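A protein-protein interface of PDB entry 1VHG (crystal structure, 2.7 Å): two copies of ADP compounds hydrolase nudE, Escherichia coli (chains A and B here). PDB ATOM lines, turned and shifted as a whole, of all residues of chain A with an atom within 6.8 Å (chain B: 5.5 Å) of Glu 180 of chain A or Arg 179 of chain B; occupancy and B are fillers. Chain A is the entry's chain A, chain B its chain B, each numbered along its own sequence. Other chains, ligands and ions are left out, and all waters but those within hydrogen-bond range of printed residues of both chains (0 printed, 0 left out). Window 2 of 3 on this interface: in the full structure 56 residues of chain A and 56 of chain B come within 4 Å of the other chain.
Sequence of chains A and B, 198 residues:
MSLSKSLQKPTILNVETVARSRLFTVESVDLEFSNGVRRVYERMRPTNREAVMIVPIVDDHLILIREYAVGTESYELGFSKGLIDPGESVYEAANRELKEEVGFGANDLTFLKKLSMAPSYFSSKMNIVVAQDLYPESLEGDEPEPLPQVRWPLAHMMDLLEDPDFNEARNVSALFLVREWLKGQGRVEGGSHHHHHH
NH2 of Arg 179 of chain A is in salt-bridge range of OE2 of Glu 180 of chain B (2.8 Å). NH1 of Arg 179 of chain B is in salt-bridge range of OE2 of Glu 180 of chain A.
NE of Arg 179 of chain B is in hydrogen-bond range of SD of Met 158 of chain B. The side-chain amino group (NZ) of Lys 183 of chain A is in salt-bridge range of the side-chain carboxylate (OE2) of Glu 180 of chain A, 3.1 Å away.
CB of Phe 176 of chain A touches CG of Phe 176 of chain B, at 3.3 Å. Glu 180 of chain B touches Phe 176 of chain A (CG to CE2, 3.7 Å). Phe 176 of chain B touches Leu 177 of chain A. Met 158 of chain B touches Glu 180 of chain A (CE to OE1, 3.97 Å). CG of Glu 180 of chain A touches CE2 of Phe 176 of chain B, at 3.5 Å.
Met 157 of chain A touches none of the printed residues of chain B. Glu 180 of chain A touches just these residues of chain B: Met 158 (3.97 Å), Phe 176 (3.5 Å) and Arg 179 (3.1 Å). Met 157 of chain B touches none of the printed residues of chain A. Printed residues of chain A within 4 Å of Met 158 of chain B: Glu 180 (3.97 Å). Printed residues of chain A within 4 Å of Phe 176 of chain B: Phe 176, Leu 177 and Glu 180. Printed residues of chain A within 4 Å of Arg 179 of chain B: Glu 180 (3.1 Å). Printed residues of chain A within 4 Å of Glu 180 of chain B: Phe 176 (3.7 Å) and Arg 179 (2.8 Å). The nearest printed residue of chain B that does not touch Glu 180 of chain A is Glu 180 of chain B (5.9 Å). The nearest residue of chain A that does not touch Arg 179 of chain B is Lys 183 of chain A (4.2 Å).
Of the 13 printed residues of chain B, 4 touch a printed residue of chain A. Of the 13 printed residues of chain A, 4 touch a printed residue of chain B. Hydrophobic or aromatic side chains of chain A within 4 Å of the printed part of chain B: Phe 176 and Leu 177. Along chain A the printed residues that touch a printed residue of chain B span positions 176 to 180.
Phe 176 of chain A touches its own counterpart, Phe 176 of chain B. Phe 176 of chain A touches Glu 180 of chain B, and with the chains exchanged Glu 180 of chain A touches Phe 176 of chain B. Leu 177 of chain A touches Phe 176 of chain B, but with the chains exchanged Phe 176 of chain A does not touch Leu 177 of chain B (4.1 Å). Arg 179 of chain A touches Glu 180 of chain B, and with the chains exchanged Glu 180 of chain A touches Arg 179 of chain B. Positions printed for both chains: 157, 174, 175, 176, 177, 178, 179, 180, 181, 182, 183 and 184. Of the 7 pairs that touch across the chains among the printed residues, 5 have their exchanged pair printed and touching as well.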
ATOM      1  N   MET A 157      16.060  -0.858  11.323  1.00  0.00           N
ATOM      2  CA  MET A 157      17.029  -0.954  10.234  1.00  0.00           C
ATOM      3  C   MET A 157      17.260  -2.390   9.723  1.00  0.00           C
ATOM      4  O   MET A 157      17.411  -2.642   8.534  1.00  0.00           O
ATOM      5  CB  MET A 157      18.402  -0.448  10.596  1.00  0.00           C
ATOM      6  CG  MET A 157      18.553   0.651  11.580  1.00  0.00           C
ATOM      7  SD  MET A 157      20.271   0.560  12.440  1.00  0.00           S
ATOM      8  CE  MET A 157      21.387   0.647  10.892  1.00  0.00           C
ATOM      9  N   ALA A 174      27.666  -1.862   5.290  1.00  0.00           N
ATOM     10  CA  ALA A 174      27.358  -0.519   5.738  1.00  0.00           C
ATOM     11  C   ALA A 174      26.319  -0.577   6.849  1.00  0.00           C
ATOM     12  O   ALA A 174      26.509   0.059   7.888  1.00  0.00           O
ATOM     13  CB  ALA A 174      26.913   0.366   4.583  1.00  0.00           C
ATOM     14  N   LEU A 175      25.222  -1.298   6.644  1.00  0.00           N
ATOM     15  CA  LEU A 175      24.154  -1.399   7.618  1.00  0.00           C
ATOM     16  C   LEU A 175      24.622  -1.839   8.994  1.00  0.00           C
ATOM     17  O   LEU A 175      24.299  -1.207   9.996  1.00  0.00           O
ATOM     18  CB  LEU A 175      23.065  -2.336   7.100  1.00  0.00           C
ATOM     19  CG  LEU A 175      21.779  -2.406   7.929  1.00  0.00           C
ATOM     20  CD1 LEU A 175      20.995  -1.100   7.808  1.00  0.00           C
ATOM     21  CD2 LEU A 175      20.923  -3.585   7.487  1.00  0.00           C
ATOM     22  N   PHE A 176      25.429  -2.891   9.085  1.00  0.00           N
ATOM     23  CA  PHE A 176      25.941  -3.420  10.330  1.00  0.00           C
ATOM     24  C   PHE A 176      26.950  -2.517  11.023  1.00  0.00           C
ATOM     25  O   PHE A 176      26.948  -2.334  12.256  1.00  0.00           O
ATOM     26  CB  PHE A 176      26.537  -4.813  10.088  1.00  0.00           C
ATOM     27  CG  PHE A 176      25.527  -5.927  10.010  1.00  0.00           C
ATOM     28  CD1 PHE A 176      25.173  -6.487   8.792  1.00  0.00           C
ATOM     29  CD2 PHE A 176      24.931  -6.417  11.163  1.00  0.00           C
ATOM     30  CE1 PHE A 176      24.250  -7.501   8.726  1.00  0.00           C
ATOM     31  CE2 PHE A 176      24.014  -7.465  11.096  1.00  0.00           C
ATOM     32  CZ  PHE A 176      23.671  -7.997   9.879  1.00  0.00           C
ATOM     33  N   LEU A 177      27.823  -1.888  10.239  1.00  0.00           N
ATOM     34  CA  LEU A 177      28.837  -0.997  10.801  1.00  0.00           C
ATOM     35  C   LEU A 177      28.186   0.262  11.330  1.00  0.00           C
ATOM     36  O   LEU A 177      28.617   0.830  12.336  1.00  0.00           O
ATOM     37  CB  LEU A 177      29.875  -0.674   9.716  1.00  0.00           C
ATOM     38  CG  LEU A 177      30.679  -1.877   9.189  1.00  0.00           C
ATOM     39  CD1 LEU A 177      31.260  -1.610   7.808  1.00  0.00           C
ATOM     40  CD2 LEU A 177      31.765  -2.237  10.172  1.00  0.00           C
ATOM     41  N   VAL A 178      27.104   0.708  10.662  1.00  0.00           N
ATOM     42  CA  VAL A 178      26.455   1.933  11.126  1.00  0.00           C
ATOM     43  C   VAL A 178      25.697   1.658  12.404  1.00  0.00           C
ATOM     44  O   VAL A 178      25.649   2.468  13.329  1.00  0.00           O
ATOM     45  CB  VAL A 178      25.604   2.601  10.061  1.00  0.00           C
ATOM     46  CG1 VAL A 178      24.928   3.849  10.637  1.00  0.00           C
ATOM     47  CG2 VAL A 178      26.445   2.989   8.855  1.00  0.00           C
ATOM     48  N   ARG A 179      25.070   0.480  12.467  1.00  0.00           N
ATOM     49  CA  ARG A 179      24.357   0.083  13.685  1.00  0.00           C
ATOM     50  C   ARG A 179      25.382  -0.087  14.798  1.00  0.00           C
ATOM     51  O   ARG A 179      25.156   0.345  15.930  1.00  0.00           O
ATOM     52  CB  ARG A 179      23.544  -1.142  13.382  1.00  0.00           C
ATOM     53  CG  ARG A 179      22.769  -1.791  14.553  1.00  0.00           C
ATOM     54  CD  ARG A 179      22.761  -3.256  14.258  1.00  0.00           C
ATOM     55  NE  ARG A 179      21.845  -4.163  14.892  1.00  0.00           N
ATOM     56  CZ  ARG A 179      22.239  -5.462  15.013  1.00  0.00           C
ATOM     57  NH1 ARG A 179      21.439  -6.344  15.584  1.00  0.00           N
ATOM     58  NH2 ARG A 179      23.427  -5.818  14.558  1.00  0.00           N
ATOM     59  N   GLU A 180      26.573  -0.639  14.534  1.00  0.00           N
ATOM     60  CA  GLU A 180      27.559  -0.748  15.612  1.00  0.00           C
ATOM     61  C   GLU A 180      27.941   0.658  16.087  1.00  0.00           C
ATOM     62  O   GLU A 180      28.061   0.898  17.282  1.00  0.00           O
ATOM     63  CB  GLU A 180      28.837  -1.468  15.229  1.00  0.00           C
ATOM     64  CG  GLU A 180      28.741  -2.957  15.059  1.00  0.00           C
ATOM     65  CD  GLU A 180      28.482  -3.647  16.383  1.00  0.00           C
ATOM     66  OE1 GLU A 180      29.270  -3.373  17.310  1.00  0.00           O
ATOM     67  OE2 GLU A 180      27.535  -4.445  16.441  1.00  0.00           O
ATOM     68  N   TRP A 181      28.186   1.546  15.132  1.00  0.00           N
ATOM     69  CA  TRP A 181      28.544   2.930  15.471  1.00  0.00           C
ATOM     70  C   TRP A 181      27.426   3.544  16.310  1.00  0.00           C
ATOM     71  O   TRP A 181      27.703   4.165  17.325  1.00  0.00           O
ATOM     72  CB  TRP A 181      28.834   3.711  14.206  1.00  0.00           C
ATOM     73  CG  TRP A 181      29.207   5.144  14.397  1.00  0.00           C
ATOM     74  CD1 TRP A 181      30.413   5.623  14.834  1.00  0.00           C
ATOM     75  CD2 TRP A 181      28.397   6.292  14.130  1.00  0.00           C
ATOM     76  NE1 TRP A 181      30.399   6.991  14.847  1.00  0.00           N
ATOM     77  CE2 TRP A 181      29.180   7.434  14.421  1.00  0.00           C
ATOM     78  CE3 TRP A 181      27.087   6.468  13.667  1.00  0.00           C
ATOM     79  CZ2 TRP A 181      28.687   8.732  14.301  1.00  0.00           C
ATOM     80  CZ3 TRP A 181      26.604   7.768  13.521  1.00  0.00           C
ATOM     81  CH2 TRP A 181      27.406   8.882  13.843  1.00  0.00           C
ATOM     82  N   LEU A 182      26.177   3.371  15.914  1.00  0.00           N
ATOM     83  CA  LEU A 182      25.010   3.851  16.634  1.00  0.00           C
ATOM     84  C   LEU A 182      24.972   3.252  18.043  1.00  0.00           C
ATOM     85  O   LEU A 182      24.770   3.932  19.042  1.00  0.00           O
ATOM     86  CB  LEU A 182      23.759   3.477  15.856  1.00  0.00           C
ATOM     87  CG  LEU A 182      23.005   4.484  15.016  1.00  0.00           C
ATOM     88  CD1 LEU A 182      23.724   5.817  14.839  1.00  0.00           C
ATOM     89  CD2 LEU A 182      22.671   3.882  13.637  1.00  0.00           C
ATOM     90  N   LYS A 183      25.201   1.934  18.146  1.00  0.00           N
ATOM     91  CA  LYS A 183      25.237   1.249  19.436  1.00  0.00           C
ATOM     92  C   LYS A 183      26.158   2.015  20.388  1.00  0.00           C
ATOM     93  O   LYS A 183      25.788   2.397  21.489  1.00  0.00           O
ATOM     94  CB  LYS A 183      25.759  -0.180  19.333  1.00  0.00           C
ATOM     95  CG  LYS A 183      24.802  -1.302  19.631  1.00  0.00           C
ATOM     96  CD  LYS A 183      25.412  -2.656  19.258  1.00  0.00           C
ATOM     97  CE  LYS A 183      24.385  -3.553  18.555  1.00  0.00           C
ATOM     98  NZ  LYS A 183      24.998  -4.873  18.215  1.00  0.00           N
ATOM     99  N   GLY A 184      27.360   2.323  19.939  1.00  0.00           N
ATOM    100  CA  GLY A 184      28.358   3.026  20.679  1.00  0.00           C
ATOM    101  C   GLY A 184      27.872   4.190  21.503  1.00  0.00           C
ATOM    102  O   GLY A 184      28.418   4.461  22.585  1.00  0.00           O
ATOM    103  N   GLN A 185      26.887   4.926  21.030  1.00  0.00           N
ATOM    104  CA  GLN A 185      26.334   6.081  21.720  1.00  0.00           C
ATOM    105  C   GLN A 185      24.874   5.896  22.092  1.00  0.00           C
ATOM    106  O   GLN A 185      24.137   6.832  22.385  1.00  0.00           O
ATOM    107  CB  GLN A 185      26.492   7.261  20.739  1.00  0.00           C
ATOM    108  CG  GLN A 185      26.299   6.813  19.299  1.00  0.00           C
ATOM    109  CD  GLN A 185      26.778   7.802  18.269  1.00  0.00           C
ATOM    110  OE1 GLN A 185      27.977   7.938  18.020  1.00  0.00           O
ATOM    111  NE2 GLN A 185      25.847   8.505  17.639  1.00  0.00           N
ATOM    112  N   MET B 157      35.713 -12.280  17.655  1.00  0.00           N
ATOM    113  CA  MET B 157      35.355 -12.176  16.250  1.00  0.00           C
ATOM    114  C   MET B 157      35.513 -10.771  15.638  1.00  0.00           C
ATOM    115  O   MET B 157      35.991 -10.593  14.537  1.00  0.00           O
ATOM    116  CB  MET B 157      33.844 -12.363  16.139  1.00  0.00           C
ATOM    117  CG  MET B 157      33.352 -13.782  16.109  1.00  0.00           C
ATOM    118  SD  MET B 157      31.427 -13.623  16.021  1.00  0.00           S
ATOM    119  CE  MET B 157      31.270 -13.771  14.103  1.00  0.00           C
ATOM    120  N   MET B 158      34.932  -9.823  16.352  1.00  0.00           N
ATOM    121  CA  MET B 158      34.885  -8.419  16.036  1.00  0.00           C
ATOM    122  C   MET B 158      36.250  -7.794  15.904  1.00  0.00           C
ATOM    123  O   MET B 158      36.356  -6.815  15.162  1.00  0.00           O
ATOM    124  CB  MET B 158      33.971  -7.678  17.010  1.00  0.00           C
ATOM    125  CG  MET B 158      32.507  -8.100  16.975  1.00  0.00           C
ATOM    126  SD  MET B 158      31.662  -7.737  15.281  1.00  0.00           S
ATOM    127  CE  MET B 158      31.637  -5.831  15.288  1.00  0.00           C
ATOM    128  N   ALA B 174      29.458 -11.310   5.966  1.00  0.00           N
ATOM    129  CA  ALA B 174      29.375 -12.637   6.553  1.00  0.00           C
ATOM    130  C   ALA B 174      29.715 -12.659   8.036  1.00  0.00           C
ATOM    131  O   ALA B 174      29.062 -13.313   8.842  1.00  0.00           O
ATOM    132  CB  ALA B 174      30.269 -13.599   5.782  1.00  0.00           C
ATOM    133  N   LEU B 175      30.702 -11.871   8.459  1.00  0.00           N
ATOM    134  CA  LEU B 175      31.063 -11.855   9.872  1.00  0.00           C
ATOM    135  C   LEU B 175      29.906 -11.338  10.711  1.00  0.00           C
ATOM    136  O   LEU B 175      29.621 -11.865  11.787  1.00  0.00           O
ATOM    137  CB  LEU B 175      32.319 -11.013  10.037  1.00  0.00           C
ATOM    138  CG  LEU B 175      32.806 -10.761  11.471  1.00  0.00           C
ATOM    139  CD1 LEU B 175      33.378 -12.031  12.076  1.00  0.00           C
ATOM    140  CD2 LEU B 175      33.853  -9.664  11.478  1.00  0.00           C
ATOM    141  N   PHE B 176      29.235 -10.272  10.256  1.00  0.00           N
ATOM    142  CA  PHE B 176      28.110  -9.727  11.005  1.00  0.00           C
ATOM    143  C   PHE B 176      26.888 -10.644  10.945  1.00  0.00           C
ATOM    144  O   PHE B 176      26.225 -10.817  11.979  1.00  0.00           O
ATOM    145  CB  PHE B 176      27.752  -8.335  10.549  1.00  0.00           C
ATOM    146  CG  PHE B 176      28.565  -7.215  11.126  1.00  0.00           C
ATOM    147  CD1 PHE B 176      29.489  -6.536  10.325  1.00  0.00           C
ATOM    148  CD2 PHE B 176      28.413  -6.813  12.440  1.00  0.00           C
ATOM    149  CE1 PHE B 176      30.221  -5.483  10.819  1.00  0.00           C
ATOM    150  CE2 PHE B 176      29.133  -5.745  12.946  1.00  0.00           C
ATOM    151  CZ  PHE B 176      30.037  -5.091  12.126  1.00  0.00           C
ATOM    152  N   LEU B 177      26.643 -11.294   9.806  1.00  0.00           N
ATOM    153  CA  LEU B 177      25.521 -12.198   9.664  1.00  0.00           C
ATOM    154  C   LEU B 177      25.700 -13.462  10.515  1.00  0.00           C
ATOM    155  O   LEU B 177      24.724 -13.998  11.072  1.00  0.00           O
ATOM    156  CB  LEU B 177      25.266 -12.566   8.199  1.00  0.00           C
ATOM    157  CG  LEU B 177      24.685 -11.459   7.309  1.00  0.00           C
ATOM    158  CD1 LEU B 177      24.970 -11.719   5.843  1.00  0.00           C
ATOM    159  CD2 LEU B 177      23.191 -11.277   7.537  1.00  0.00           C
ATOM    160  N   VAL B 178      26.952 -13.910  10.656  1.00  0.00           N
ATOM    161  CA  VAL B 178      27.204 -15.121  11.435  1.00  0.00           C
ATOM    162  C   VAL B 178      27.020 -14.792  12.906  1.00  0.00           C
ATOM    163  O   VAL B 178      26.477 -15.564  13.702  1.00  0.00           O
ATOM    164  CB  VAL B 178      28.572 -15.737  11.139  1.00  0.00           C
ATOM    165  CG1 VAL B 178      28.944 -16.799  12.161  1.00  0.00           C
ATOM    166  CG2 VAL B 178      28.639 -16.341   9.725  1.00  0.00           C
ATOM    167  N   ARG B 179      27.482 -13.595  13.285  1.00  0.00           N
ATOM    168  CA  ARG B 179      27.342 -13.165  14.676  1.00  0.00           C
ATOM    169  C   ARG B 179      25.874 -12.990  15.018  1.00  0.00           C
ATOM    170  O   ARG B 179      25.476 -13.505  16.079  1.00  0.00           O
ATOM    171  CB  ARG B 179      28.231 -11.997  14.964  1.00  0.00           C
ATOM    172  CG  ARG B 179      27.909 -11.123  16.179  1.00  0.00           C
ATOM    173  CD  ARG B 179      29.164 -10.385  16.546  1.00  0.00           C
ATOM    174  NE  ARG B 179      29.079  -9.143  17.247  1.00  0.00           N
ATOM    175  CZ  ARG B 179      28.432  -8.033  16.972  1.00  0.00           C
ATOM    176  NH1 ARG B 179      28.557  -7.014  17.802  1.00  0.00           N
ATOM    177  NH2 ARG B 179      27.657  -7.895  15.913  1.00  0.00           N
ATOM    178  N   GLU B 180      25.033 -12.393  14.159  1.00  0.00           N
ATOM    179  CA  GLU B 180      23.605 -12.282  14.510  1.00  0.00           C
ATOM    180  C   GLU B 180      23.039 -13.710  14.722  1.00  0.00           C
ATOM    181  O   GLU B 180      22.285 -13.969  15.637  1.00  0.00           O
ATOM    182  CB  GLU B 180      22.707 -11.610  13.498  1.00  0.00           C
ATOM    183  CG  GLU B 180      22.689 -10.143  13.304  1.00  0.00           C
ATOM    184  CD  GLU B 180      22.640  -9.315  14.559  1.00  0.00           C
ATOM    185  OE1 GLU B 180      21.610  -9.330  15.258  1.00  0.00           O
ATOM    186  OE2 GLU B 180      23.632  -8.617  14.840  1.00  0.00           O
ATOM    187  N   TRP B 181      23.372 -14.604  13.812  1.00  0.00           N
ATOM    188  CA  TRP B 181      22.937 -15.986  13.908  1.00  0.00           C
ATOM    189  C   TRP B 181      23.433 -16.607  15.201  1.00  0.00           C
ATOM    190  O   TRP B 181      22.680 -17.257  15.921  1.00  0.00           O
ATOM    191  CB  TRP B 181      23.392 -16.719  12.655  1.00  0.00           C
ATOM    192  CG  TRP B 181      23.055 -18.171  12.637  1.00  0.00           C
ATOM    193  CD1 TRP B 181      21.824 -18.717  12.397  1.00  0.00           C
ATOM    194  CD2 TRP B 181      23.944 -19.266  12.905  1.00  0.00           C
ATOM    195  NE1 TRP B 181      21.895 -20.077  12.491  1.00  0.00           N
ATOM    196  CE2 TRP B 181      23.185 -20.451  12.779  1.00  0.00           C
ATOM    197  CE3 TRP B 181      25.290 -19.367  13.220  1.00  0.00           C
ATOM    198  CZ2 TRP B 181      23.732 -21.720  12.944  1.00  0.00           C
ATOM    199  CZ3 TRP B 181      25.832 -20.634  13.417  1.00  0.00           C
ATOM    200  CH2 TRP B 181      25.058 -21.805  13.278  1.00  0.00           C
ATOM    201  N   LEU B 182      24.690 -16.425  15.585  1.00  0.00           N
ATOM    202  CA  LEU B 182      25.222 -16.971  16.835  1.00  0.00           C
ATOM    203  C   LEU B 182      24.479 -16.379  18.043  1.00  0.00           C
ATOM    204  O   LEU B 182      24.297 -17.018  19.084  1.00  0.00           O
ATOM    205  CB  LEU B 182      26.696 -16.641  16.918  1.00  0.00           C
ATOM    206  CG  LEU B 182      27.805 -17.616  16.673  1.00  0.00           C
ATOM    207  CD1 LEU B 182      27.369 -18.869  15.935  1.00  0.00           C
ATOM    208  CD2 LEU B 182      28.956 -16.929  15.906  1.00  0.00           C
ATOM    209  N   LYS B 183      24.146 -15.091  17.961  1.00  0.00           N
ATOM    210  CA  LYS B 183      23.422 -14.393  19.015  1.00  0.00           C
ATOM    211  C   LYS B 183      22.112 -15.154  19.247  1.00  0.00           C
ATOM    212  O   LYS B 183      21.717 -15.475  20.354  1.00  0.00           O
ATOM    213  CB  LYS B 183      23.093 -12.961  18.602  1.00  0.00           C
ATOM    214  CG  LYS B 183      23.791 -11.872  19.379  1.00  0.00           C
ATOM    215  N   GLY B 184      21.463 -15.475  18.136  1.00  0.00           N
ATOM    216  CA  GLY B 184      20.226 -16.221  18.111  1.00  0.00           C
ATOM    217  C   GLY B 184      20.257 -17.340  19.141  1.00  0.00           C
ATOM    218  O   GLY B 184      19.398 -17.363  20.027  1.00  0.00           O
